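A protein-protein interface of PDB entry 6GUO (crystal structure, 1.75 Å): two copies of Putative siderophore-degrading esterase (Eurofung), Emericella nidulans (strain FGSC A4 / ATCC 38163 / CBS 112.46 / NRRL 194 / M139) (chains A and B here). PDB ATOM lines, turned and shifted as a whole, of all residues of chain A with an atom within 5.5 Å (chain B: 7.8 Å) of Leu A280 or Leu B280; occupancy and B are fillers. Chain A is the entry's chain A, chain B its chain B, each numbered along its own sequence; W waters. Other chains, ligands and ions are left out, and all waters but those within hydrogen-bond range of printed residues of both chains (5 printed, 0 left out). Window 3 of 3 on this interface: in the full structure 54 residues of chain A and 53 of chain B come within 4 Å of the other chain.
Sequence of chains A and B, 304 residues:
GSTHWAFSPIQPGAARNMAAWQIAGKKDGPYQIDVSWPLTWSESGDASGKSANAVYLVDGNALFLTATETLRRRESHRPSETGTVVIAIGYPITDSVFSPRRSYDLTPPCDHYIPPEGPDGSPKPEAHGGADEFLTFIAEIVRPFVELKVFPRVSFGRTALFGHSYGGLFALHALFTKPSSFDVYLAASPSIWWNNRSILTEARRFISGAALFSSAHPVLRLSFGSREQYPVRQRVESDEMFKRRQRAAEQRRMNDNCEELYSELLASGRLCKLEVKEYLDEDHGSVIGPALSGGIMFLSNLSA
N of Asp A281 lies within hydrogen-bond range of OG of Ser A226, 2.8 Å away.
The backbone NH of Ser A226 lies within hydrogen-bond range of the backbone carbonyl oxygen of Glu A282 (3.4 Å).
The backbone carbonyl oxygen (O) of Tyr B279 lies within hydrogen-bond range of the backbone NH (N) of Ser B226, 2.9 Å away.
N of Asp B281 sits at hydrogen-bond distance from OG of Ser B226 (2.7 Å).
O of Asp B281 is in hydrogen-bond range of NE of Arg B227, 3.3 Å away.
The side-chain carboxylate (OE1) of Glu B282 sits at hydrogen-bond distance from the side-chain hydroxyl (OG) of Ser B286, at 2.7 Å.
Lys A277 touches Leu B280, and with the chains exchanged Leu A280 touches Lys B277.
Lys A277 touches Asp B281, and with the chains exchanged Asp A281 touches Lys B277.
Tyr A279 touches Glu B282, and with the chains exchanged Glu A282 touches Tyr B279.
Leu B280 touches its own counterpart, Leu A280.
Of the 7 pairs that touch across the chains among the printed residues, 7 have their exchanged pair printed and touching as well.
Of the 7 printed residues of chain A, 5 touch a printed residue of chain B.
Of the 14 printed residues of chain B, 5 touch a printed residue of chain A.
Printed residues of chain B that touch a printed residue of chain A: Lys B277, Tyr B279, Leu B280, Asp B281 and Glu B282.
Water W1 lies within hydrogen-bond range of OE2 of Glu B282 (2.5 Å) and OH of Tyr A279 (2.9 Å).
Water W5 bridges OE2 of Glu A282 (2.6 Å) and O of Pro B290 (2.7 Å).
Water W2 lies within hydrogen-bond range of O of Leu A280 (2.6 Å) and NZ of Lys B277 (3.0 Å).
Water W3 bridges the backbone carbonyl oxygen (O) of Leu B280 (2.7 Å) and the side-chain amino group (NZ) of Lys A277 (2.8 Å).
Water W4 lies within hydrogen-bond range of OH of Tyr B279 (2.7 Å) and OE2 of Glu A282 (3.1 Å).
The side-chain amino group (NZ) of Lys A277 lies within hydrogen-bond range of the backbone carbonyl oxygen (O) of Leu B280, at 3.3 Å.
NZ of Lys A277 is in salt-bridge range of OD2 of Asp B281, 3.3 Å away.
The side-chain carboxylate (OD2) of Asp A281 lies within salt-bridge range of the side-chain amino group (NZ) of Lys B277 (3.6 Å).
Leu A280 touches two residues of chain B.
Printed residues of chain A within 4 Å of Leu B280: Lys A277 and Leu A280.
Of the printed residues of chain B, Asp A281 touches Lys B277 (3.6 Å).
Printed residues of chain A within 4 Å of Glu B282: Tyr A279.
Of the printed residues of chain A, Lys B277 touches Leu A280 and Asp A281.
Gly B225 touches none of the printed residues of chain A.
Among the printed residues, pairs that only touch across the chains: Tyr A279 with Glu B282 (3.9 Å), Leu A280 with Lys B277 (3.5 Å), Leu A280 with Leu B280 (3.4 Å) and Glu A282 with Tyr B279 (3.999 Å).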
ATOM      1  N   SER A 226      -4.590   4.324  14.934  1.00  0.00           N
ATOM      2  CA  SER A 226      -5.039   3.193  15.764  1.00  0.00           C
ATOM      3  C   SER A 226      -5.711   3.631  17.069  1.00  0.00           C
ATOM      4  O   SER A 226      -6.619   2.956  17.556  1.00  0.00           O
ATOM      5  CB  SER A 226      -3.884   2.227  16.068  1.00  0.00           C
ATOM      6  OG  SER A 226      -2.972   2.785  17.002  1.00  0.00           O
ATOM      7  N   LYS A 277      -5.099   2.156   5.395  1.00  0.00           N
ATOM      8  CA  LYS A 277      -3.896   2.178   6.232  1.00  0.00           C
ATOM      9  C   LYS A 277      -4.264   2.588   7.653  1.00  0.00           C
ATOM     10  O   LYS A 277      -4.852   3.650   7.867  1.00  0.00           O
ATOM     11  CB  LYS A 277      -2.858   3.146   5.646  1.00  0.00           C
ATOM     12  CG  LYS A 277      -1.613   3.393   6.499  1.00  0.00           C
ATOM     13  CD  LYS A 277      -0.774   2.140   6.703  1.00  0.00           C
ATOM     14  CE  LYS A 277       0.310   2.351   7.755  1.00  0.00           C
ATOM     15  NZ  LYS A 277       1.533   3.004   7.222  1.00  0.00           N
ATOM     16  N   GLU A 278      -3.918   1.734   8.613  1.00  0.00           N
ATOM     17  CA  GLU A 278      -4.004   2.060  10.027  1.00  0.00           C
ATOM     18  C   GLU A 278      -2.638   2.573  10.445  1.00  0.00           C
ATOM     19  O   GLU A 278      -1.642   1.865  10.276  1.00  0.00           O
ATOM     20  CB  GLU A 278      -4.359   0.820  10.851  1.00  0.00           C
ATOM     21  CG  GLU A 278      -4.376   1.053  12.358  1.00  0.00           C
ATOM     22  CD  GLU A 278      -4.896  -0.141  13.137  1.00  0.00           C
ATOM     23  OE1 GLU A 278      -5.414   0.061  14.253  1.00  0.00           O
ATOM     24  OE2 GLU A 278      -4.780  -1.283  12.645  1.00  0.00           O
ATOM     25  N   TYR A 279      -2.592   3.788  10.986  1.00  0.00           N
ATOM     26  CA  TYR A 279      -1.344   4.366  11.487  1.00  0.00           C
ATOM     27  C   TYR A 279      -1.219   4.057  12.975  1.00  0.00           C
ATOM     28  O   TYR A 279      -1.955   4.608  13.789  1.00  0.00           O
ATOM     29  CB  TYR A 279      -1.293   5.876  11.222  1.00  0.00           C
ATOM     30  CG  TYR A 279      -1.024   6.202   9.773  1.00  0.00           C
ATOM     31  CD1 TYR A 279       0.275   6.232   9.286  1.00  0.00           C
ATOM     32  CD2 TYR A 279      -2.068   6.457   8.881  1.00  0.00           C
ATOM     33  CE1 TYR A 279       0.541   6.518   7.960  1.00  0.00           C
ATOM     34  CE2 TYR A 279      -1.813   6.740   7.546  1.00  0.00           C
ATOM     35  CZ  TYR A 279      -0.505   6.767   7.091  1.00  0.00           C
ATOM     36  OH  TYR A 279      -0.225   7.041   5.782  1.00  0.00           O
ATOM     37  N   LEU A 280      -0.292   3.165  13.324  1.00  0.00           N
ATOM     38  CA  LEU A 280      -0.146   2.719  14.710  1.00  0.00           C
ATOM     39  C   LEU A 280       0.257   3.858  15.640  1.00  0.00           C
ATOM     40  O   LEU A 280       1.119   4.671  15.303  1.00  0.00           O
ATOM     41  CB  LEU A 280       0.881   1.587  14.822  1.00  0.00           C
ATOM     42  CG  LEU A 280       0.526   0.219  14.247  1.00  0.00           C
ATOM     43  CD1 LEU A 280       1.660  -0.754  14.547  1.00  0.00           C
ATOM     44  CD2 LEU A 280      -0.792  -0.311  14.804  1.00  0.00           C
ATOM     45  N   ASP A 281      -0.401   3.911  16.799  1.00  0.00           N
ATOM     46  CA  ASP A 281      -0.113   4.868  17.878  1.00  0.00           C
ATOM     47  C   ASP A 281      -0.460   6.329  17.580  1.00  0.00           C
ATOM     48  O   ASP A 281      -0.112   7.213  18.366  1.00  0.00           O
ATOM     49  CB  ASP A 281       1.359   4.783  18.338  1.00  0.00           C
ATOM     50  CG  ASP A 281       1.843   3.357  18.521  1.00  0.00           C
ATOM     51  OD1 ASP A 281       1.085   2.509  19.044  1.00  0.00           O
ATOM     52  OD2 ASP A 281       2.998   3.088  18.137  1.00  0.00           O
ATOM     53  N   GLU A 282      -1.164   6.592  16.478  1.00  0.00           N
ATOM     54  CA  GLU A 282      -1.578   7.952  16.144  1.00  0.00           C
ATOM     55  C   GLU A 282      -3.028   8.160  16.564  1.00  0.00           C
ATOM     56  O   GLU A 282      -3.845   7.238  16.496  1.00  0.00           O
ATOM     57  CB  GLU A 282      -1.421   8.236  14.650  1.00  0.00           C
ATOM     58  CG  GLU A 282      -0.040   7.943  14.070  1.00  0.00           C
ATOM     59  CD  GLU A 282       1.060   8.902  14.506  1.00  0.00           C
ATOM     60  OE1 GLU A 282       0.830   9.818  15.325  1.00  0.00           O
ATOM     61  OE2 GLU A 282       2.189   8.731  14.004  1.00  0.00           O
ATOM     62  N   PHE B 224      12.847   5.169  12.705  1.00  0.00           N
ATOM     63  CA  PHE B 224      13.154   4.682  11.364  1.00  0.00           C
ATOM     64  C   PHE B 224      11.894   4.125  10.714  1.00  0.00           C
ATOM     65  O   PHE B 224      10.911   3.820  11.394  1.00  0.00           O
ATOM     66  CB  PHE B 224      14.244   3.600  11.414  1.00  0.00           C
ATOM     67  CG  PHE B 224      13.874   2.407  12.251  1.00  0.00           C
ATOM     68  CD1 PHE B 224      13.300   1.283  11.668  1.00  0.00           C
ATOM     69  CD2 PHE B 224      14.093   2.409  13.626  1.00  0.00           C
ATOM     70  CE1 PHE B 224      12.948   0.184  12.436  1.00  0.00           C
ATOM     71  CE2 PHE B 224      13.741   1.315  14.399  1.00  0.00           C
ATOM     72  CZ  PHE B 224      13.168   0.199  13.803  1.00  0.00           C
ATOM     73  N   GLY B 225      11.934   3.993   9.395  1.00  0.00           N
ATOM     74  CA  GLY B 225      10.868   3.346   8.639  1.00  0.00           C
ATOM     75  C   GLY B 225      11.165   1.867   8.479  1.00  0.00           C
ATOM     76  O   GLY B 225      12.317   1.485   8.219  1.00  0.00           O
ATOM     77  N   SER B 226      10.137   1.028   8.610  1.00  0.00           N
ATOM     78  CA  SER B 226      10.324  -0.432   8.557  1.00  0.00           C
ATOM     79  C   SER B 226      10.948  -0.911   7.236  1.00  0.00           C
ATOM     80  O   SER B 226      11.737  -1.861   7.228  1.00  0.00           O
ATOM     81  CB  SER B 226       9.003  -1.171   8.831  1.00  0.00           C
ATOM     82  OG  SER B 226       8.091  -1.031   7.759  1.00  0.00           O
ATOM     83  N   ARG B 227      10.624  -0.232   6.134  1.00  0.00           N
ATOM     84  CA  ARG B 227      11.160  -0.582   4.811  1.00  0.00           C
ATOM     85  C   ARG B 227      12.614  -0.156   4.547  1.00  0.00           C
ATOM     86  O   ARG B 227      13.181  -0.529   3.518  1.00  0.00           O
ATOM     87  CB  ARG B 227      10.263  -0.021   3.704  1.00  0.00           C
ATOM     88  CG  ARG B 227       8.878  -0.621   3.721  1.00  0.00           C
ATOM     89  CD  ARG B 227       8.062  -0.127   2.547  1.00  0.00           C
ATOM     90  NE  ARG B 227       6.752  -0.764   2.522  1.00  0.00           N
ATOM     91  CZ  ARG B 227       5.799  -0.506   1.628  1.00  0.00           C
ATOM     92  NH1 ARG B 227       5.994   0.390   0.664  1.00  0.00           N
ATOM     93  NH2 ARG B 227       4.636  -1.149   1.704  1.00  0.00           N
ATOM     94  N   LYS B 277      10.987   4.429  17.829  1.00  0.00           N
ATOM     95  CA  LYS B 277       9.741   4.204  17.102  1.00  0.00           C
ATOM     96  C   LYS B 277      10.046   3.710  15.702  1.00  0.00           C
ATOM     97  O   LYS B 277      10.793   4.354  14.958  1.00  0.00           O
ATOM     98  CB  LYS B 277       8.918   5.495  17.024  1.00  0.00           C
ATOM     99  CG  LYS B 277       7.679   5.429  16.129  1.00  0.00           C
ATOM    100  CD  LYS B 277       6.694   4.359  16.576  1.00  0.00           C
ATOM    101  CE  LYS B 277       5.472   4.295  15.666  1.00  0.00           C
ATOM    102  NZ  LYS B 277       4.513   5.406  15.892  1.00  0.00           N
ATOM    103  N   GLU B 278       9.455   2.570  15.358  1.00  0.00           N
ATOM    104  CA  GLU B 278       9.464   2.048  14.002  1.00  0.00           C
ATOM    105  C   GLU B 278       8.162   2.467  13.321  1.00  0.00           C
ATOM    106  O   GLU B 278       7.075   2.162  13.817  1.00  0.00           O
ATOM    107  CB  GLU B 278       9.568   0.523  14.023  1.00  0.00           C
ATOM    108  CG  GLU B 278       9.488  -0.130  12.645  1.00  0.00           C
ATOM    109  CD  GLU B 278       9.775  -1.617  12.680  1.00  0.00           C
ATOM    110  OE1 GLU B 278       9.979  -2.198  11.602  1.00  0.00           O
ATOM    111  OE2 GLU B 278       9.792  -2.213  13.776  1.00  0.00           O
ATOM    112  N   TYR B 279       8.282   3.161  12.195  1.00  0.00           N
ATOM    113  CA  TYR B 279       7.121   3.542  11.392  1.00  0.00           C
ATOM    114  C   TYR B 279       6.895   2.488  10.322  1.00  0.00           C
ATOM    115  O   TYR B 279       7.661   2.398   9.355  1.00  0.00           O
ATOM    116  CB  TYR B 279       7.325   4.922  10.778  1.00  0.00           C
ATOM    117  CG  TYR B 279       7.240   6.026  11.801  1.00  0.00           C
ATOM    118  CD1 TYR B 279       6.005   6.560  12.169  1.00  0.00           C
ATOM    119  CD2 TYR B 279       8.384   6.533  12.415  1.00  0.00           C
ATOM    120  CE1 TYR B 279       5.910   7.568  13.114  1.00  0.00           C
ATOM    121  CE2 TYR B 279       8.299   7.545  13.366  1.00  0.00           C
ATOM    122  CZ  TYR B 279       7.062   8.063  13.702  1.00  0.00           C
ATOM    123  OH  TYR B 279       6.973   9.054  14.641  1.00  0.00           O
ATOM    124  N   LEU B 280       5.856   1.678  10.519  1.00  0.00           N
ATOM    125  CA  LEU B 280       5.555   0.567   9.617  1.00  0.00           C
ATOM    126  C   LEU B 280       5.242   1.045   8.209  1.00  0.00           C
ATOM    127  O   LEU B 280       4.568   2.064   8.024  1.00  0.00           O
ATOM    128  CB  LEU B 280       4.366  -0.255  10.127  1.00  0.00           C
ATOM    129  CG  LEU B 280       4.529  -1.019  11.437  1.00  0.00           C
ATOM    130  CD1 LEU B 280       3.257  -1.805  11.713  1.00  0.00           C
ATOM    131  CD2 LEU B 280       5.737  -1.950  11.405  1.00  0.00           C
ATOM    132  N   ASP B 281       5.747   0.295   7.229  1.00  0.00           N
ATOM    133  CA  ASP B 281       5.520   0.546   5.796  1.00  0.00           C
ATOM    134  C   ASP B 281       6.222   1.786   5.225  1.00  0.00           C
ATOM    135  O   ASP B 281       6.070   2.060   4.039  1.00  0.00           O
ATOM    136  CB  ASP B 281       4.022   0.620   5.451  1.00  0.00           C
ATOM    137  CG  ASP B 281       3.207  -0.486   6.096  1.00  0.00           C
ATOM    138  OD1 ASP B 281       3.611  -1.664   6.001  1.00  0.00           O
ATOM    139  OD2 ASP B 281       2.157  -0.167   6.697  1.00  0.00           O
ATOM    140  N   GLU B 282       6.984   2.527   6.028  1.00  0.00           N
ATOM    141  CA  GLU B 282       7.615   3.747   5.540  1.00  0.00           C
ATOM    142  C   GLU B 282       9.038   3.454   5.093  1.00  0.00           C
ATOM    143  O   GLU B 282       9.714   2.605   5.674  1.00  0.00           O
ATOM    144  CB  GLU B 282       7.614   4.850   6.603  1.00  0.00           C
ATOM    145  CG  GLU B 282       6.251   5.191   7.199  1.00  0.00           C
ATOM    146  CD  GLU B 282       5.274   5.856   6.236  1.00  0.00           C
ATOM    147  OE1 GLU B 282       5.546   5.975   5.021  1.00  0.00           O
ATOM    148  OE2 GLU B 282       4.204   6.273   6.720  1.00  0.00           O
ATOM    149  N   ASP B 283       9.480   4.165   4.059  1.00  0.00           N
ATOM    150  CA  ASP B 283      10.850   4.044   3.536  1.00  0.00           C
ATOM    151  C   ASP B 283      11.652   5.286   3.931  1.00  0.00           C
ATOM    152  O   ASP B 283      11.152   6.134   4.675  1.00  0.00           O
ATOM    153  CB  ASP B 283      10.844   3.767   2.015  1.00  0.00           C
ATOM    154  CG  ASP B 283      10.204   4.884   1.191  1.00  0.00           C
ATOM    155  OD1 ASP B 283      10.273   6.066   1.576  1.00  0.00           O
ATOM    156  OD2 ASP B 283       9.631   4.568   0.128  1.00  0.00           O
ATOM    157  N   SER B 286       9.707   8.465   2.731  1.00  0.00           N
ATOM    158  CA  SER B 286       8.318   8.553   3.205  1.00  0.00           C
ATOM    159  C   SER B 286       8.194   8.692   4.730  1.00  0.00           C
ATOM    160  O   SER B 286       7.198   9.215   5.216  1.00  0.00           O
ATOM    161  CB  SER B 286       7.484   7.366   2.708  1.00  0.00           C
ATOM    162  OG  SER B 286       7.749   6.186   3.441  1.00  0.00           O
ATOM    163  N   VAL B 287       9.204   8.235   5.472  1.00  0.00           N
ATOM    164  CA  VAL B 287       9.205   8.343   6.935  1.00  0.00           C
ATOM    165  C   VAL B 287       9.465   9.762   7.463  1.00  0.00           C
ATOM    166  O   VAL B 287       9.185  10.032   8.632  1.00  0.00           O
ATOM    167  CB  VAL B 287      10.226   7.348   7.572  1.00  0.00           C
ATOM    168  CG1 VAL B 287      11.657   7.863   7.453  1.00  0.00           C
ATOM    169  CG2 VAL B 287       9.861   7.051   9.022  1.00  0.00           C
ATOM    170  N   PRO B 290       6.170  11.653   8.882  1.00  0.00           N
ATOM    171  CA  PRO B 290       5.723  10.963  10.089  1.00  0.00           C
ATOM    172  C   PRO B 290       6.684  11.104  11.278  1.00  0.00           C
ATOM    173  O   PRO B 290       6.238  11.375  12.390  1.00  0.00           O
ATOM    174  CB  PRO B 290       5.623   9.507   9.638  1.00  0.00           C
ATOM    175  CG  PRO B 290       5.312   9.585   8.187  1.00  0.00           C
ATOM    176  CD  PRO B 290       6.000  10.816   7.679  1.00  0.00           C
HETATM  177  O   HOH W   1       2.574   7.951   5.791  1.00  0.00           O
HETATM  178  O   HOH W   2       2.944   4.792  13.400  1.00  0.00           O
HETATM  179  O   HOH W   3       2.987   3.666   9.533  1.00  0.00           O
HETATM  180  O   HOH W   4       4.601   9.038  15.963  1.00  0.00           O
HETATM  181  O   HOH W   5       3.813  10.684  13.459  1.00  0.00           O
